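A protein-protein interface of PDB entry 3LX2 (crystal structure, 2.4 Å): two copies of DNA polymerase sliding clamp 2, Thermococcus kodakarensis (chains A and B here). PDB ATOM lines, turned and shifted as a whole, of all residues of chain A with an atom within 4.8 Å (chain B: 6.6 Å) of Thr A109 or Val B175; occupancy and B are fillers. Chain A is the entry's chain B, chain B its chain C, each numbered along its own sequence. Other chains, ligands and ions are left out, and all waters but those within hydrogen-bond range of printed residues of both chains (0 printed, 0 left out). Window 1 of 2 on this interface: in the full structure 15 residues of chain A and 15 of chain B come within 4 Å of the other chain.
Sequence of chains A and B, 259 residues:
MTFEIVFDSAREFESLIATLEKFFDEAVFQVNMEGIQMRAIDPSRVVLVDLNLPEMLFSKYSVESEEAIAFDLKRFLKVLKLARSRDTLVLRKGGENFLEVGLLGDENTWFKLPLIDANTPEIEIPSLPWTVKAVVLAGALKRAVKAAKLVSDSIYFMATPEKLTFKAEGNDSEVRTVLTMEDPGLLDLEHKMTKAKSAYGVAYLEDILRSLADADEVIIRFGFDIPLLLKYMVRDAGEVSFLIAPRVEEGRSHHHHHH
No position is printed for both chains. Of the 15 pairs that touch across the chains among the printed residues, none has its exchanged pair printed and touching as well.
The backbone carbonyl oxygen (O) of Val B175 is in hydrogen-bond range of the backbone NH (N) of Ala B168, at 3.0 Å. The backbone NH (N) of Thr B177 sits at hydrogen-bond distance from the backbone carbonyl oxygen (O) of Phe B166. The backbone carbonyl oxygen of Val A101 is in hydrogen-bond range of the backbone NH of Phe A111, 2.7 Å away. The backbone NH (N) of Leu A103 sits at hydrogen-bond distance from the backbone carbonyl oxygen (O) of Thr A109, 2.7 Å away.
Hydrophobic or aromatic side chains of chain A within 4 Å of the printed part of chain B: Trp A110 and Phe A111. Among the printed residues, Asp or Glu carboxylates within 4 Å of a Lys or Arg side-chain nitrogen of the other chain: Glu A107 with Arg B143.
NH1 of Arg B143 lies within hydrogen-bond range of OG1 of Thr A109, 2.7 Å away. The backbone NH of Trp A110 is in hydrogen-bond range of the backbone carbonyl oxygen of Arg B176, at 3.0 Å. The backbone carbonyl oxygen (O) of Asn A108 sits at hydrogen-bond distance from the backbone NH (N) of Val B178 (3.2 Å). The side-chain hydroxyl (OG1) of Thr A109 is in hydrogen-bond range of the side-chain hydroxyl (OG1) of Thr B177 (3.3 Å). NE of Arg B143 lies within salt-bridge range of OE1 of Glu A107 (3.96 Å).
Val A101 touches none of the printed residues of chain B. Printed residues of chain B within 4 Å of Asn A108: Arg B176, Thr B177 and Val B178. Of chain B, only Arg B143, Val B175, Arg B176 and Thr B177 come within 4 Å of Thr A109. Of the printed residues of chain B, Phe A111 touches Ala B147, Leu B150, Glu B174 and Val B175. Of the printed residues of chain A, Ala B147 touches Phe A111. Of chain A, only Thr A109, Trp A110 and Phe A111 come within 4 Å of Val B175. Of the printed residues of chain A, Arg B176 touches Asn A108 (3.9 Å), Thr A109 (3.4 Å) and Trp A110 (3.0 Å).
Among the printed residues, pairs that only touch across the chains: Trp A110 with Val B175, Phe A111 with Glu B174, Asn A108 with Thr B177, Thr A109 with Arg B176, Phe A111 with Val B175, Thr A109 with Val B175, Trp A110 with Glu B174, Phe A111 with Leu B150, Asn A108 with Arg B176 and Phe A111 with Ala B147.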
ATOM      1  N   VAL A 101      20.649 -11.656  19.913  1.00  0.00           N
ATOM      2  CA  VAL A 101      20.581 -13.020  19.356  1.00  0.00           C
ATOM      3  C   VAL A 101      20.999 -13.097  17.875  1.00  0.00           C
ATOM      4  O   VAL A 101      20.361 -12.543  16.978  1.00  0.00           O
ATOM      5  CB  VAL A 101      19.163 -13.671  19.522  1.00  0.00           C
ATOM      6  CG1 VAL A 101      19.191 -15.120  19.013  1.00  0.00           C
ATOM      7  CG2 VAL A 101      18.709 -13.635  20.975  1.00  0.00           C
ATOM      8  N   GLY A 102      22.061 -13.831  17.624  1.00  0.00           N
ATOM      9  CA  GLY A 102      22.582 -13.907  16.272  1.00  0.00           C
ATOM     10  C   GLY A 102      22.461 -15.308  15.727  1.00  0.00           C
ATOM     11  O   GLY A 102      22.859 -16.245  16.408  1.00  0.00           O
ATOM     12  N   LEU A 103      21.916 -15.433  14.514  1.00  0.00           N
ATOM     13  CA  LEU A 103      21.897 -16.673  13.737  1.00  0.00           C
ATOM     14  C   LEU A 103      22.847 -16.535  12.536  1.00  0.00           C
ATOM     15  O   LEU A 103      22.489 -15.938  11.520  1.00  0.00           O
ATOM     16  CB  LEU A 103      20.449 -16.991  13.296  1.00  0.00           C
ATOM     17  CG  LEU A 103      19.422 -17.199  14.439  1.00  0.00           C
ATOM     18  CD1 LEU A 103      18.065 -17.549  13.934  1.00  0.00           C
ATOM     19  CD2 LEU A 103      19.882 -18.253  15.432  1.00  0.00           C
ATOM     20  N   LEU A 104      24.061 -17.076  12.657  1.00  0.00           N
ATOM     21  CA  LEU A 104      25.119 -16.771  11.686  1.00  0.00           C
ATOM     22  C   LEU A 104      25.355 -17.870  10.652  1.00  0.00           C
ATOM     23  O   LEU A 104      25.715 -19.016  10.998  1.00  0.00           O
ATOM     24  CB  LEU A 104      26.424 -16.382  12.369  1.00  0.00           C
ATOM     25  CG  LEU A 104      26.413 -15.289  13.427  1.00  0.00           C
ATOM     26  CD1 LEU A 104      27.828 -14.860  13.681  1.00  0.00           C
ATOM     27  CD2 LEU A 104      25.595 -14.114  13.011  1.00  0.00           C
ATOM     28  N   GLU A 107      22.918 -16.300   5.627  1.00  0.00           N
ATOM     29  CA  GLU A 107      22.442 -14.987   6.051  1.00  0.00           C
ATOM     30  C   GLU A 107      22.922 -14.761   7.480  1.00  0.00           C
ATOM     31  O   GLU A 107      23.110 -15.710   8.221  1.00  0.00           O
ATOM     32  CB  GLU A 107      20.910 -14.960   5.985  1.00  0.00           C
ATOM     33  CG  GLU A 107      20.325 -15.419   4.595  1.00  0.00           C
ATOM     34  CD  GLU A 107      19.723 -16.868   4.552  1.00  0.00           C
ATOM     35  OE1 GLU A 107      19.315 -17.458   5.603  1.00  0.00           O
ATOM     36  OE2 GLU A 107      19.633 -17.412   3.425  1.00  0.00           O
ATOM     37  N   ASN A 108      23.189 -13.524   7.862  1.00  0.00           N
ATOM     38  CA  ASN A 108      23.443 -13.224   9.256  1.00  0.00           C
ATOM     39  C   ASN A 108      22.193 -12.543   9.760  1.00  0.00           C
ATOM     40  O   ASN A 108      21.705 -11.614   9.122  1.00  0.00           O
ATOM     41  CB  ASN A 108      24.659 -12.329   9.420  1.00  0.00           C
ATOM     42  CG  ASN A 108      25.969 -13.101   9.350  1.00  0.00           C
ATOM     43  OD1 ASN A 108      26.000 -14.274   8.986  1.00  0.00           O
ATOM     44  ND2 ASN A 108      27.061 -12.442   9.712  1.00  0.00           N
ATOM     45  N   THR A 109      21.628 -13.036  10.859  1.00  0.00           N
ATOM     46  CA  THR A 109      20.464 -12.372  11.434  1.00  0.00           C
ATOM     47  C   THR A 109      20.630 -12.102  12.903  1.00  0.00           C
ATOM     48  O   THR A 109      20.993 -12.998  13.651  1.00  0.00           O
ATOM     49  CB  THR A 109      19.197 -13.154  11.220  1.00  0.00           C
ATOM     50  OG1 THR A 109      19.041 -13.404   9.818  1.00  0.00           O
ATOM     51  CG2 THR A 109      18.020 -12.359  11.732  1.00  0.00           C
ATOM     52  N   TRP A 110      20.333 -10.861  13.290  1.00  0.00           N
ATOM     53  CA  TRP A 110      20.475 -10.382  14.665  1.00  0.00           C
ATOM     54  C   TRP A 110      19.158  -9.880  15.265  1.00  0.00           C
ATOM     55  O   TRP A 110      18.461  -9.043  14.656  1.00  0.00           O
ATOM     56  CB  TRP A 110      21.508  -9.278  14.672  1.00  0.00           C
ATOM     57  CG  TRP A 110      22.858  -9.810  14.476  1.00  0.00           C
ATOM     58  CD1 TRP A 110      23.560  -9.900  13.296  1.00  0.00           C
ATOM     59  CD2 TRP A 110      23.693 -10.391  15.491  1.00  0.00           C
ATOM     60  NE1 TRP A 110      24.802 -10.485  13.527  1.00  0.00           N
ATOM     61  CE2 TRP A 110      24.906 -10.791  14.862  1.00  0.00           C
ATOM     62  CE3 TRP A 110      23.536 -10.603  16.867  1.00  0.00           C
ATOM     63  CZ2 TRP A 110      25.949 -11.371  15.563  1.00  0.00           C
ATOM     64  CZ3 TRP A 110      24.580 -11.202  17.575  1.00  0.00           C
ATOM     65  CH2 TRP A 110      25.775 -11.580  16.910  1.00  0.00           C
ATOM     66  N   PHE A 111      18.784 -10.404  16.426  1.00  0.00           N
ATOM     67  CA  PHE A 111      17.635  -9.840  17.125  1.00  0.00           C
ATOM     68  C   PHE A 111      18.111  -9.110  18.366  1.00  0.00           C
ATOM     69  O   PHE A 111      19.129  -9.461  18.957  1.00  0.00           O
ATOM     70  CB  PHE A 111      16.630 -10.903  17.565  1.00  0.00           C
ATOM     71  CG  PHE A 111      15.893 -11.574  16.440  1.00  0.00           C
ATOM     72  CD1 PHE A 111      16.495 -12.585  15.690  1.00  0.00           C
ATOM     73  CD2 PHE A 111      14.598 -11.231  16.166  1.00  0.00           C
ATOM     74  CE1 PHE A 111      15.818 -13.209  14.659  1.00  0.00           C
ATOM     75  CE2 PHE A 111      13.893 -11.865  15.129  1.00  0.00           C
ATOM     76  CZ  PHE A 111      14.497 -12.860  14.383  1.00  0.00           C
ATOM     77  N   ARG B 143      13.904 -15.587   4.482  1.00  0.00           N
ATOM     78  CA  ARG B 143      14.473 -15.397   5.774  1.00  0.00           C
ATOM     79  C   ARG B 143      14.131 -13.993   6.161  1.00  0.00           C
ATOM     80  O   ARG B 143      13.416 -13.784   7.142  1.00  0.00           O
ATOM     81  CB  ARG B 143      15.998 -15.574   5.750  1.00  0.00           C
ATOM     82  CG  ARG B 143      16.752 -14.937   6.928  1.00  0.00           C
ATOM     83  CD  ARG B 143      16.291 -15.460   8.290  1.00  0.00           C
ATOM     84  NE  ARG B 143      16.814 -16.803   8.598  1.00  0.00           N
ATOM     85  CZ  ARG B 143      18.008 -17.039   9.146  1.00  0.00           C
ATOM     86  NH1 ARG B 143      18.843 -16.027   9.432  1.00  0.00           N
ATOM     87  NH2 ARG B 143      18.373 -18.288   9.383  1.00  0.00           N
ATOM     88  N   ALA B 144      14.598 -13.035   5.367  1.00  0.00           N
ATOM     89  CA  ALA B 144      14.462 -11.628   5.718  1.00  0.00           C
ATOM     90  C   ALA B 144      13.058 -11.339   6.252  1.00  0.00           C
ATOM     91  O   ALA B 144      12.878 -10.802   7.381  1.00  0.00           O
ATOM     92  CB  ALA B 144      14.731 -10.767   4.511  1.00  0.00           C
ATOM     93  N   ALA B 147      11.928 -13.365   9.461  1.00  0.00           N
ATOM     94  CA  ALA B 147      12.566 -12.721  10.565  1.00  0.00           C
ATOM     95  C   ALA B 147      11.831 -11.423  10.902  1.00  0.00           C
ATOM     96  O   ALA B 147      11.655 -11.093  12.059  1.00  0.00           O
ATOM     97  CB  ALA B 147      14.006 -12.412  10.206  1.00  0.00           C
ATOM     98  N   ALA B 148      11.408 -10.670   9.893  1.00  0.00           N
ATOM     99  CA  ALA B 148      10.776  -9.390  10.202  1.00  0.00           C
ATOM    100  C   ALA B 148       9.407  -9.574  10.872  1.00  0.00           C
ATOM    101  O   ALA B 148       9.124  -8.899  11.826  1.00  0.00           O
ATOM    102  CB  ALA B 148      10.730  -8.466   8.985  1.00  0.00           C
ATOM    103  N   LYS B 149       8.607 -10.529  10.404  1.00  0.00           N
ATOM    104  CA  LYS B 149       7.247 -10.769  10.894  1.00  0.00           C
ATOM    105  C   LYS B 149       7.209 -10.884  12.420  1.00  0.00           C
ATOM    106  O   LYS B 149       6.260 -10.462  13.051  1.00  0.00           O
ATOM    107  CB  LYS B 149       6.709 -12.050  10.243  1.00  0.00           C
ATOM    108  CG  LYS B 149       5.192 -12.300  10.347  1.00  0.00           C
ATOM    109  CD  LYS B 149       4.781 -13.630   9.629  1.00  0.00           C
ATOM    110  CE  LYS B 149       3.256 -13.917   9.695  1.00  0.00           C
ATOM    111  NZ  LYS B 149       2.803 -15.235   9.028  1.00  0.00           N
ATOM    112  N   LEU B 150       8.263 -11.431  13.004  1.00  0.00           N
ATOM    113  CA  LEU B 150       8.323 -11.697  14.435  1.00  0.00           C
ATOM    114  C   LEU B 150       8.403 -10.441  15.268  1.00  0.00           C
ATOM    115  O   LEU B 150       8.378 -10.477  16.524  1.00  0.00           O
ATOM    116  CB  LEU B 150       9.608 -12.436  14.703  1.00  0.00           C
ATOM    117  CG  LEU B 150       9.563 -13.942  14.834  1.00  0.00           C
ATOM    118  CD1 LEU B 150       8.945 -14.618  13.662  1.00  0.00           C
ATOM    119  CD2 LEU B 150      10.994 -14.402  15.044  1.00  0.00           C
ATOM    120  N   VAL B 151       8.569  -9.324  14.573  1.00  0.00           N
ATOM    121  CA  VAL B 151       8.869  -8.087  15.231  1.00  0.00           C
ATOM    122  C   VAL B 151       7.921  -7.005  14.745  1.00  0.00           C
ATOM    123  O   VAL B 151       7.682  -6.065  15.473  1.00  0.00           O
ATOM    124  CB  VAL B 151      10.369  -7.719  15.067  1.00  0.00           C
ATOM    125  CG1 VAL B 151      10.601  -6.254  15.292  1.00  0.00           C
ATOM    126  CG2 VAL B 151      11.237  -8.501  16.048  1.00  0.00           C
ATOM    127  N   SER B 152       7.335  -7.140  13.549  1.00  0.00           N
ATOM    128  CA  SER B 152       6.546  -6.038  12.987  1.00  0.00           C
ATOM    129  C   SER B 152       5.770  -6.380  11.744  1.00  0.00           C
ATOM    130  O   SER B 152       6.065  -7.370  11.047  1.00  0.00           O
ATOM    131  CB  SER B 152       7.434  -4.825  12.650  1.00  0.00           C
ATOM    132  OG  SER B 152       6.772  -3.976  11.695  1.00  0.00           O
ATOM    133  N   THR B 165      20.411  -4.576   3.717  1.00  0.00           N
ATOM    134  CA  THR B 165      19.882  -4.762   5.039  1.00  0.00           C
ATOM    135  C   THR B 165      18.369  -4.764   5.027  1.00  0.00           C
ATOM    136  O   THR B 165      17.741  -3.889   4.403  1.00  0.00           O
ATOM    137  CB  THR B 165      20.318  -3.661   5.957  1.00  0.00           C
ATOM    138  OG1 THR B 165      21.734  -3.621   5.960  1.00  0.00           O
ATOM    139  CG2 THR B 165      19.831  -3.932   7.365  1.00  0.00           C
ATOM    140  N   PHE B 166      17.806  -5.759   5.721  1.00  0.00           N
ATOM    141  CA  PHE B 166      16.374  -5.923   5.875  1.00  0.00           C
ATOM    142  C   PHE B 166      16.150  -5.854   7.372  1.00  0.00           C
ATOM    143  O   PHE B 166      16.622  -6.725   8.118  1.00  0.00           O
ATOM    144  CB  PHE B 166      15.950  -7.278   5.325  1.00  0.00           C
ATOM    145  CG  PHE B 166      16.329  -7.497   3.893  1.00  0.00           C
ATOM    146  CD1 PHE B 166      17.525  -8.099   3.572  1.00  0.00           C
ATOM    147  CD2 PHE B 166      15.488  -7.088   2.870  1.00  0.00           C
ATOM    148  CE1 PHE B 166      17.901  -8.279   2.249  1.00  0.00           C
ATOM    149  CE2 PHE B 166      15.853  -7.246   1.544  1.00  0.00           C
ATOM    150  CZ  PHE B 166      17.064  -7.871   1.229  1.00  0.00           C
ATOM    151  N   LYS B 167      15.482  -4.791   7.811  1.00  0.00           N
ATOM    152  CA  LYS B 167      15.434  -4.410   9.225  1.00  0.00           C
ATOM    153  C   LYS B 167      13.978  -4.200   9.590  1.00  0.00           C
ATOM    154  O   LYS B 167      13.144  -3.980   8.709  1.00  0.00           O
ATOM    155  CB  LYS B 167      16.191  -3.101   9.404  1.00  0.00           C
ATOM    156  CG  LYS B 167      16.667  -2.772  10.829  1.00  0.00           C
ATOM    157  CD  LYS B 167      17.560  -1.488  10.859  1.00  0.00           C
ATOM    158  CE  LYS B 167      17.885  -0.978  12.310  1.00  0.00           C
ATOM    159  NZ  LYS B 167      19.080  -1.597  13.018  1.00  0.00           N
ATOM    160  N   ALA B 168      13.656  -4.280  10.881  1.00  0.00           N
ATOM    161  CA  ALA B 168      12.279  -4.035  11.352  1.00  0.00           C
ATOM    162  C   ALA B 168      12.305  -3.736  12.834  1.00  0.00           C
ATOM    163  O   ALA B 168      13.259  -4.116  13.507  1.00  0.00           O
ATOM    164  CB  ALA B 168      11.392  -5.237  11.072  1.00  0.00           C
ATOM    165  N   GLU B 169      11.283  -3.048  13.346  1.00  0.00           N
ATOM    166  CA  GLU B 169      11.169  -2.856  14.805  1.00  0.00           C
ATOM    167  C   GLU B 169       9.788  -2.605  15.437  1.00  0.00           C
ATOM    168  O   GLU B 169       8.765  -2.568  14.758  1.00  0.00           O
ATOM    169  CB  GLU B 169      12.145  -1.782  15.270  1.00  0.00           C
ATOM    170  CG  GLU B 169      11.880  -0.451  14.640  1.00  0.00           C
ATOM    171  CD  GLU B 169      12.001   0.636  15.644  1.00  0.00           C
ATOM    172  OE1 GLU B 169      13.157   1.063  15.890  1.00  0.00           O
ATOM    173  OE2 GLU B 169      10.939   1.033  16.193  1.00  0.00           O
ATOM    174  N   SER B 173      11.513  -4.643  20.424  1.00  0.00           N
ATOM    175  CA  SER B 173      12.601  -5.453  19.869  1.00  0.00           C
ATOM    176  C   SER B 173      12.984  -5.000  18.455  1.00  0.00           C
ATOM    177  O   SER B 173      12.258  -4.217  17.828  1.00  0.00           O
ATOM    178  CB  SER B 173      12.172  -6.921  19.855  1.00  0.00           C
ATOM    179  OG  SER B 173      10.915  -7.074  19.229  1.00  0.00           O
ATOM    180  N   GLU B 174      14.120  -5.485  17.959  1.00  0.00           N
ATOM    181  CA  GLU B 174      14.506  -5.236  16.560  1.00  0.00           C
ATOM    182  C   GLU B 174      15.189  -6.433  15.908  1.00  0.00           C
ATOM    183  O   GLU B 174      15.555  -7.412  16.579  1.00  0.00           O
ATOM    184  CB  GLU B 174      15.374  -3.973  16.418  1.00  0.00           C
ATOM    185  CG  GLU B 174      16.728  -4.000  17.131  1.00  0.00           C
ATOM    186  CD  GLU B 174      17.439  -2.637  17.106  1.00  0.00           C
ATOM    187  OE1 GLU B 174      16.724  -1.626  17.273  1.00  0.00           O
ATOM    188  OE2 GLU B 174      18.691  -2.572  16.927  1.00  0.00           O
ATOM    189  N   VAL B 175      15.392  -6.342  14.598  1.00  0.00           N
ATOM    190  CA  VAL B 175      15.972  -7.444  13.856  1.00  0.00           C
ATOM    191  C   VAL B 175      16.473  -6.967  12.527  1.00  0.00           C
ATOM    192  O   VAL B 175      15.737  -6.311  11.772  1.00  0.00           O
ATOM    193  CB  VAL B 175      14.946  -8.553  13.603  1.00  0.00           C
ATOM    194  CG1 VAL B 175      13.734  -8.016  12.833  1.00  0.00           C
ATOM    195  CG2 VAL B 175      15.596  -9.718  12.898  1.00  0.00           C
ATOM    196  N   ARG B 176      17.725  -7.308  12.251  1.00  0.00           N
ATOM    197  CA  ARG B 176      18.333  -7.026  10.972  1.00  0.00           C
ATOM    198  C   ARG B 176      18.880  -8.287  10.352  1.00  0.00           C
ATOM    199  O   ARG B 176      19.432  -9.150  11.040  1.00  0.00           O
ATOM    200  CB  ARG B 176      19.433  -5.978  11.111  1.00  0.00           C
ATOM    201  CG  ARG B 176      20.536  -6.379  12.044  1.00  0.00           C
ATOM    202  CD  ARG B 176      21.599  -5.317  12.118  1.00  0.00           C
ATOM    203  NE  ARG B 176      22.490  -5.542  13.265  1.00  0.00           N
ATOM    204  CZ  ARG B 176      23.725  -6.024  13.180  1.00  0.00           C
ATOM    205  NH1 ARG B 176      24.231  -6.347  11.987  1.00  0.00           N
ATOM    206  NH2 ARG B 176      24.452  -6.183  14.294  1.00  0.00           N
ATOM    207  N   THR B 177      18.684  -8.389   9.049  1.00  0.00           N
ATOM    208  CA  THR B 177      19.294  -9.413   8.237  1.00  0.00           C
ATOM    209  C   THR B 177      20.168  -8.692   7.201  1.00  0.00           C
ATOM    210  O   THR B 177      19.728  -7.809   6.463  1.00  0.00           O
ATOM    211  CB  THR B 177      18.238 -10.280   7.511  1.00  0.00           C
ATOM    212  OG1 THR B 177      17.348 -10.908   8.455  1.00  0.00           O
ATOM    213  CG2 THR B 177      18.911 -11.327   6.657  1.00  0.00           C
ATOM    214  N   VAL B 178      21.412  -9.107   7.145  1.00  0.00           N
ATOM    215  CA  VAL B 178      22.399  -8.447   6.357  1.00  0.00           C
ATOM    216  C   VAL B 178      22.898  -9.388   5.274  1.00  0.00           C
ATOM    217  O   VAL B 178      23.142 -10.561   5.497  1.00  0.00           O
ATOM    218  CB  VAL B 178      23.507  -7.936   7.273  1.00  0.00           C
ATOM    219  CG1 VAL B 178      24.830  -7.742   6.538  1.00  0.00           C
ATOM    220  CG2 VAL B 178      23.050  -6.634   7.876  1.00  0.00           C
